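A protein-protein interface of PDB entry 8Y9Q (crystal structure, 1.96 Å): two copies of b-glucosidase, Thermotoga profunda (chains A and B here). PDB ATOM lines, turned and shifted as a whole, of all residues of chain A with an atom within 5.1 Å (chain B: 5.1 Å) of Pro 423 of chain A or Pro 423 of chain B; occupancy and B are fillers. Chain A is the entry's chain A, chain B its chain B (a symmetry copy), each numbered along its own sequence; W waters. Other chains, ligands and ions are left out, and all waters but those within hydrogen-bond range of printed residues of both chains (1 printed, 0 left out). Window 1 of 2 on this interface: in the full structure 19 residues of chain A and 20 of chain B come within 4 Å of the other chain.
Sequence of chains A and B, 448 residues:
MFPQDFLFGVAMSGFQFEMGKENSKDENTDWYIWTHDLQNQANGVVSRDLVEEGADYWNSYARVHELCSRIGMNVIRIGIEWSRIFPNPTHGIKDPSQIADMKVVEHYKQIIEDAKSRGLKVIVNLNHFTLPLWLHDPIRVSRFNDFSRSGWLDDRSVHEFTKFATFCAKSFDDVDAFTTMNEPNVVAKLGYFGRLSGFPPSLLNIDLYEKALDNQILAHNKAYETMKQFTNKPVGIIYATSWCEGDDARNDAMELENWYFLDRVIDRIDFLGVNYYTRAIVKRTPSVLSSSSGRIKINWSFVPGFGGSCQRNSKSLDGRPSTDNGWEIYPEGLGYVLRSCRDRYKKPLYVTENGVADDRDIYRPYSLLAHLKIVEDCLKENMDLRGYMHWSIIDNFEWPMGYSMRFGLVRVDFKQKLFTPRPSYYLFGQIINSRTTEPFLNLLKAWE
Of chain A, only Pro 365 and Pro 423 come within 4 Å of Pro 423 of chain B. Of the printed residues of chain B, Pro 421 of chain A touches Leu 443 (3.6 Å). Of the printed residues of chain A, Pro 365 of chain B touches Pro 423. Tyr 425 of chain B touches none of the printed residues of chain A. Ser 424 of chain A touches none of the printed residues of chain B. The nearest printed residue of chain A that does not touch Arg 422 of chain B is Leu 427 of chain A (6.2 Å).
Hydrophobic or aromatic side chains of chain A that line the printed part of chain B: Pro 365, Pro 423, Tyr 426 and Leu 443. Of the 10 printed residues of chain B, 6 touch a printed residue of chain A. Hydrophobic or aromatic side chains of chain B within 4 Å of the printed part of chain A: Pro 365, Pro 423, Tyr 426 and Leu 443. Among the printed residues, 8 pairs touch across the chains. Among the printed residues, no Asp or Glu carboxylate lies within 4 Å of a Lys or Arg side-chain nitrogen of the other chain.
Pro 365 of chain A touches Pro 423 of chain B (CB to CG, 3.9 Å). O of Pro 421 of chain A touches CD1 of Leu 443 of chain B (3.6 Å). Leu 443 of chain B touches Arg 422 of chain A. Pro 423 of chain A touches Pro 365 of chain B (CG to CB, 3.9 Å). Pro 423 of chain A touches Pro 423 of chain B. CB of Tyr 426 of chain A touches CB of Tyr 426 of chain B, at 3.9 Å. Leu 443 of chain A touches Pro 421 of chain B. Leu 443 of chain A touches Arg 422 of chain B.
Water W1 bridges the backbone carbonyl oxygen (O) of Asp 361 of chain A and the backbone carbonyl oxygen (O) of Asp 361 of chain B.
Pro 365 of chain A touches Pro 423 of chain B, and with the chains exchanged Pro 423 of chain A touches Pro 365 of chain B. Pro 421 of chain A touches Leu 443 of chain B, and with the chains exchanged Leu 443 of chain A touches Pro 421 of chain B. Pro 423 of chain A touches its own counterpart, Pro 423 of chain B. Tyr 426 of chain B touches its own counterpart, Tyr 426 of chain A. 10 positions are printed for both chains.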
ATOM      1  N   ASP A 361      -2.803 -25.252  18.032  1.00  0.00           N
ATOM      2  CA  ASP A 361      -4.002 -24.751  17.352  1.00  0.00           C
ATOM      3  C   ASP A 361      -4.251 -25.459  16.023  1.00  0.00           C
ATOM      4  O   ASP A 361      -4.790 -24.864  15.091  1.00  0.00           O
ATOM      5  CB  ASP A 361      -3.961 -23.223  17.145  1.00  0.00           C
ATOM      6  CG  ASP A 361      -5.359 -22.578  17.173  1.00  0.00           C
ATOM      7  OD1 ASP A 361      -6.110 -22.808  18.151  1.00  0.00           O
ATOM      8  OD2 ASP A 361      -5.687 -21.789  16.249  1.00  0.00           O
ATOM      9  N   PRO A 365      -9.395 -24.753  15.419  1.00  0.00           N
ATOM     10  CA  PRO A 365     -10.226 -24.131  14.363  1.00  0.00           C
ATOM     11  C   PRO A 365     -11.247 -25.092  13.776  1.00  0.00           C
ATOM     12  O   PRO A 365     -12.424 -24.746  13.653  1.00  0.00           O
ATOM     13  CB  PRO A 365      -9.199 -23.674  13.317  1.00  0.00           C
ATOM     14  CG  PRO A 365      -7.927 -23.472  14.096  1.00  0.00           C
ATOM     15  CD  PRO A 365      -7.957 -24.480  15.222  1.00  0.00           C
ATOM     16  N   PRO A 421      -3.441 -14.576  21.726  1.00  0.00           N
ATOM     17  CA  PRO A 421      -4.505 -15.308  21.019  1.00  0.00           C
ATOM     18  C   PRO A 421      -3.971 -16.210  19.908  1.00  0.00           C
ATOM     19  O   PRO A 421      -3.075 -15.837  19.149  1.00  0.00           O
ATOM     20  CB  PRO A 421      -5.388 -14.189  20.457  1.00  0.00           C
ATOM     21  CG  PRO A 421      -5.142 -13.015  21.423  1.00  0.00           C
ATOM     22  CD  PRO A 421      -3.700 -13.125  21.795  1.00  0.00           C
ATOM     23  N   ARG A 422      -4.531 -17.415  19.834  1.00  0.00           N
ATOM     24  CA  ARG A 422      -4.265 -18.327  18.728  1.00  0.00           C
ATOM     25  C   ARG A 422      -5.180 -17.969  17.565  1.00  0.00           C
ATOM     26  O   ARG A 422      -6.147 -17.229  17.744  1.00  0.00           O
ATOM     27  CB  ARG A 422      -4.503 -19.773  19.153  1.00  0.00           C
ATOM     28  CG  ARG A 422      -3.629 -20.242  20.316  1.00  0.00           C
ATOM     29  CD  ARG A 422      -3.972 -21.689  20.719  1.00  0.00           C
ATOM     30  NE  ARG A 422      -2.959 -22.274  21.602  1.00  0.00           N
ATOM     31  CZ  ARG A 422      -3.014 -22.252  22.932  1.00  0.00           C
ATOM     32  NH1 ARG A 422      -4.052 -21.733  23.577  1.00  0.00           N
ATOM     33  NH2 ARG A 422      -1.993 -22.743  23.632  1.00  0.00           N
ATOM     34  N   PRO A 423      -4.898 -18.466  16.356  1.00  0.00           N
ATOM     35  CA  PRO A 423      -5.757 -18.097  15.218  1.00  0.00           C
ATOM     36  C   PRO A 423      -7.208 -18.497  15.412  1.00  0.00           C
ATOM     37  O   PRO A 423      -8.096 -17.803  14.909  1.00  0.00           O
ATOM     38  CB  PRO A 423      -5.109 -18.835  14.037  1.00  0.00           C
ATOM     39  CG  PRO A 423      -3.674 -18.906  14.410  1.00  0.00           C
ATOM     40  CD  PRO A 423      -3.668 -19.149  15.909  1.00  0.00           C
ATOM     41  N   SER A 424      -7.478 -19.581  16.148  1.00  0.00           N
ATOM     42  CA  SER A 424      -8.866 -19.961  16.421  1.00  0.00           C
ATOM     43  C   SER A 424      -9.632 -18.860  17.158  1.00  0.00           C
ATOM     44  O   SER A 424     -10.861 -18.775  17.044  1.00  0.00           O
ATOM     45  CB  SER A 424      -8.907 -21.271  17.228  1.00  0.00           C
ATOM     46  OG  SER A 424      -8.096 -21.177  18.400  1.00  0.00           O
ATOM     47  N   TYR A 425      -8.935 -18.030  17.944  1.00  0.00           N
ATOM     48  CA  TYR A 425      -9.587 -16.898  18.605  1.00  0.00           C
ATOM     49  C   TYR A 425     -10.152 -15.926  17.577  1.00  0.00           C
ATOM     50  O   TYR A 425     -11.301 -15.485  17.682  1.00  0.00           O
ATOM     51  CB  TYR A 425      -8.585 -16.197  19.527  1.00  0.00           C
ATOM     52  CG  TYR A 425      -9.015 -14.853  20.116  1.00  0.00           C
ATOM     53  CD1 TYR A 425      -9.704 -14.789  21.331  1.00  0.00           C
ATOM     54  CD2 TYR A 425      -8.668 -13.654  19.492  1.00  0.00           C
ATOM     55  CE1 TYR A 425     -10.068 -13.559  21.894  1.00  0.00           C
ATOM     56  CE2 TYR A 425      -9.019 -12.416  20.043  1.00  0.00           C
ATOM     57  CZ  TYR A 425      -9.722 -12.376  21.239  1.00  0.00           C
ATOM     58  OH  TYR A 425     -10.067 -11.154  21.770  1.00  0.00           O
ATOM     59  N   TYR A 426      -9.355 -15.590  16.557  1.00  0.00           N
ATOM     60  CA  TYR A 426      -9.842 -14.690  15.513  1.00  0.00           C
ATOM     61  C   TYR A 426     -10.943 -15.342  14.681  1.00  0.00           C
ATOM     62  O   TYR A 426     -11.871 -14.654  14.245  1.00  0.00           O
ATOM     63  CB  TYR A 426      -8.673 -14.238  14.633  1.00  0.00           C
ATOM     64  CG  TYR A 426      -7.575 -13.574  15.443  1.00  0.00           C
ATOM     65  CD1 TYR A 426      -7.809 -12.378  16.116  1.00  0.00           C
ATOM     66  CD2 TYR A 426      -6.323 -14.164  15.572  1.00  0.00           C
ATOM     67  CE1 TYR A 426      -6.813 -11.777  16.884  1.00  0.00           C
ATOM     68  CE2 TYR A 426      -5.323 -13.571  16.337  1.00  0.00           C
ATOM     69  CZ  TYR A 426      -5.579 -12.381  16.987  1.00  0.00           C
ATOM     70  OH  TYR A 426      -4.591 -11.797  17.745  1.00  0.00           O
ATOM     71  N   LEU A 427     -10.874 -16.660  14.466  1.00  0.00           N
ATOM     72  CA  LEU A 427     -11.942 -17.330  13.729  1.00  0.00           C
ATOM     73  C   LEU A 427     -13.258 -17.284  14.508  1.00  0.00           C
ATOM     74  O   LEU A 427     -14.319 -17.007  13.932  1.00  0.00           O
ATOM     75  CB  LEU A 427     -11.540 -18.779  13.406  1.00  0.00           C
ATOM     76  CG  LEU A 427     -12.644 -19.607  12.732  1.00  0.00           C
ATOM     77  CD1 LEU A 427     -12.961 -19.067  11.348  1.00  0.00           C
ATOM     78  CD2 LEU A 427     -12.270 -21.097  12.658  1.00  0.00           C
ATOM     79  N   LEU A 443     -14.197 -24.758   4.795  1.00  0.00           N
ATOM     80  CA  LEU A 443     -12.969 -25.153   5.490  1.00  0.00           C
ATOM     81  C   LEU A 443     -13.040 -26.593   5.979  1.00  0.00           C
ATOM     82  O   LEU A 443     -12.007 -27.271   6.080  1.00  0.00           O
ATOM     83  CB  LEU A 443     -12.693 -24.226   6.680  1.00  0.00           C
ATOM     84  CG  LEU A 443     -12.430 -22.747   6.366  1.00  0.00           C
ATOM     85  CD1 LEU A 443     -12.095 -21.966   7.630  1.00  0.00           C
ATOM     86  CD2 LEU A 443     -11.320 -22.596   5.304  1.00  0.00           C
ATOM     87  N   ASP B 361      -4.711 -25.870   7.044  1.00  0.00           N
ATOM     88  CA  ASP B 361      -4.165 -24.694   7.733  1.00  0.00           C
ATOM     89  C   ASP B 361      -3.463 -25.082   9.036  1.00  0.00           C
ATOM     90  O   ASP B 361      -3.434 -24.311  10.000  1.00  0.00           O
ATOM     91  CB  ASP B 361      -5.243 -23.625   7.993  1.00  0.00           C
ATOM     92  CG  ASP B 361      -4.676 -22.196   7.977  1.00  0.00           C
ATOM     93  OD1 ASP B 361      -3.910 -21.862   7.041  1.00  0.00           O
ATOM     94  OD2 ASP B 361      -5.013 -21.396   8.877  1.00  0.00           O
ATOM     95  N   PRO B 365      -0.182 -20.971   9.730  1.00  0.00           N
ATOM     96  CA  PRO B 365      -0.015 -19.969  10.802  1.00  0.00           C
ATOM     97  C   PRO B 365       1.384 -19.970  11.385  1.00  0.00           C
ATOM     98  O   PRO B 365       2.014 -18.914  11.518  1.00  0.00           O
ATOM     99  CB  PRO B 365      -1.067 -20.387  11.841  1.00  0.00           C
ATOM    100  CG  PRO B 365      -2.106 -21.111  11.051  1.00  0.00           C
ATOM    101  CD  PRO B 365      -1.364 -21.830   9.955  1.00  0.00           C
ATOM    102  N   PRO B 421     -11.625 -17.649   3.607  1.00  0.00           N
ATOM    103  CA  PRO B 421     -10.353 -17.453   4.324  1.00  0.00           C
ATOM    104  C   PRO B 421     -10.098 -18.506   5.403  1.00  0.00           C
ATOM    105  O   PRO B 421     -10.995 -18.880   6.165  1.00  0.00           O
ATOM    106  CB  PRO B 421     -10.522 -16.058   4.943  1.00  0.00           C
ATOM    107  CG  PRO B 421     -11.418 -15.345   3.962  1.00  0.00           C
ATOM    108  CD  PRO B 421     -12.419 -16.407   3.543  1.00  0.00           C
ATOM    109  N   ARG B 422      -8.847 -18.967   5.472  1.00  0.00           N
ATOM    110  CA  ARG B 422      -8.388 -19.834   6.549  1.00  0.00           C
ATOM    111  C   ARG B 422      -7.953 -18.975   7.730  1.00  0.00           C
ATOM    112  O   ARG B 422      -7.740 -17.773   7.578  1.00  0.00           O
ATOM    113  CB  ARG B 422      -7.216 -20.695   6.060  1.00  0.00           C
ATOM    114  CG  ARG B 422      -7.588 -21.698   4.947  1.00  0.00           C
ATOM    115  CD  ARG B 422      -6.334 -22.468   4.470  1.00  0.00           C
ATOM    116  NE  ARG B 422      -6.669 -23.574   3.576  1.00  0.00           N
ATOM    117  CZ  ARG B 422      -6.623 -23.512   2.250  1.00  0.00           C
ATOM    118  NH1 ARG B 422      -6.221 -22.415   1.619  1.00  0.00           N
ATOM    119  NH2 ARG B 422      -7.003 -24.570   1.539  1.00  0.00           N
ATOM    120  N   PRO B 423      -7.805 -19.554   8.925  1.00  0.00           N
ATOM    121  CA  PRO B 423      -7.443 -18.708  10.083  1.00  0.00           C
ATOM    122  C   PRO B 423      -6.107 -17.969   9.932  1.00  0.00           C
ATOM    123  O   PRO B 423      -5.965 -16.854  10.457  1.00  0.00           O
ATOM    124  CB  PRO B 423      -7.429 -19.702  11.253  1.00  0.00           C
ATOM    125  CG  PRO B 423      -8.437 -20.771  10.829  1.00  0.00           C
ATOM    126  CD  PRO B 423      -8.213 -20.917   9.326  1.00  0.00           C
ATOM    127  N   SER B 424      -5.138 -18.548   9.215  1.00  0.00           N
ATOM    128  CA  SER B 424      -3.870 -17.868   8.936  1.00  0.00           C
ATOM    129  C   SER B 424      -4.088 -16.537   8.220  1.00  0.00           C
ATOM    130  O   SER B 424      -3.283 -15.608   8.362  1.00  0.00           O
ATOM    131  CB  SER B 424      -2.983 -18.779   8.081  1.00  0.00           C
ATOM    132  OG  SER B 424      -3.670 -19.153   6.886  1.00  0.00           O
ATOM    133  N   TYR B 425      -5.162 -16.432   7.438  1.00  0.00           N
ATOM    134  CA  TYR B 425      -5.512 -15.155   6.823  1.00  0.00           C
ATOM    135  C   TYR B 425      -5.772 -14.085   7.879  1.00  0.00           C
ATOM    136  O   TYR B 425      -5.275 -12.953   7.775  1.00  0.00           O
ATOM    137  CB  TYR B 425      -6.729 -15.359   5.929  1.00  0.00           C
ATOM    138  CG  TYR B 425      -7.383 -14.126   5.339  1.00  0.00           C
ATOM    139  CD1 TYR B 425      -6.975 -13.613   4.102  1.00  0.00           C
ATOM    140  CD2 TYR B 425      -8.456 -13.522   5.978  1.00  0.00           C
ATOM    141  CE1 TYR B 425      -7.609 -12.495   3.546  1.00  0.00           C
ATOM    142  CE2 TYR B 425      -9.109 -12.437   5.433  1.00  0.00           C
ATOM    143  CZ  TYR B 425      -8.694 -11.931   4.211  1.00  0.00           C
ATOM    144  OH  TYR B 425      -9.344 -10.818   3.699  1.00  0.00           O
ATOM    145  N   TYR B 426      -6.562 -14.419   8.908  1.00  0.00           N
ATOM    146  CA  TYR B 426      -6.844 -13.422   9.939  1.00  0.00           C
ATOM    147  C   TYR B 426      -5.609 -13.131  10.775  1.00  0.00           C
ATOM    148  O   TYR B 426      -5.413 -11.991  11.212  1.00  0.00           O
ATOM    149  CB  TYR B 426      -8.020 -13.876  10.820  1.00  0.00           C
ATOM    150  CG  TYR B 426      -9.263 -14.172  10.008  1.00  0.00           C
ATOM    151  CD1 TYR B 426      -9.993 -13.149   9.409  1.00  0.00           C
ATOM    152  CD2 TYR B 426      -9.682 -15.476   9.807  1.00  0.00           C
ATOM    153  CE1 TYR B 426     -11.109 -13.424   8.630  1.00  0.00           C
ATOM    154  CE2 TYR B 426     -10.802 -15.764   9.040  1.00  0.00           C
ATOM    155  CZ  TYR B 426     -11.510 -14.731   8.454  1.00  0.00           C
ATOM    156  OH  TYR B 426     -12.613 -15.021   7.679  1.00  0.00           O
ATOM    157  N   LEU B 427      -4.762 -14.135  11.001  1.00  0.00           N
ATOM    158  CA  LEU B 427      -3.510 -13.891  11.711  1.00  0.00           C
ATOM    159  C   LEU B 427      -2.621 -12.921  10.942  1.00  0.00           C
ATOM    160  O   LEU B 427      -2.004 -12.027  11.539  1.00  0.00           O
ATOM    161  CB  LEU B 427      -2.771 -15.210  11.944  1.00  0.00           C
ATOM    162  CG  LEU B 427      -1.365 -15.099  12.550  1.00  0.00           C
ATOM    163  CD1 LEU B 427      -1.430 -14.458  13.941  1.00  0.00           C
ATOM    164  CD2 LEU B 427      -0.703 -16.478  12.620  1.00  0.00           C
ATOM    165  N   LEU B 443       3.308 -17.807  20.403  1.00  0.00           N
ATOM    166  CA  LEU B 443       2.690 -18.918  19.688  1.00  0.00           C
ATOM    167  C   LEU B 443       3.741 -19.909  19.197  1.00  0.00           C
ATOM    168  O   LEU B 443       3.481 -21.118  19.144  1.00  0.00           O
ATOM    169  CB  LEU B 443       1.879 -18.386  18.504  1.00  0.00           C
ATOM    170  CG  LEU B 443       0.690 -17.484  18.877  1.00  0.00           C
ATOM    171  CD1 LEU B 443      -0.079 -17.045  17.629  1.00  0.00           C
ATOM    172  CD2 LEU B 443      -0.243 -18.178  19.869  1.00  0.00           C
HETATM  173  O   HOH W   1      -3.706 -24.367  12.718  1.00  0.00           O
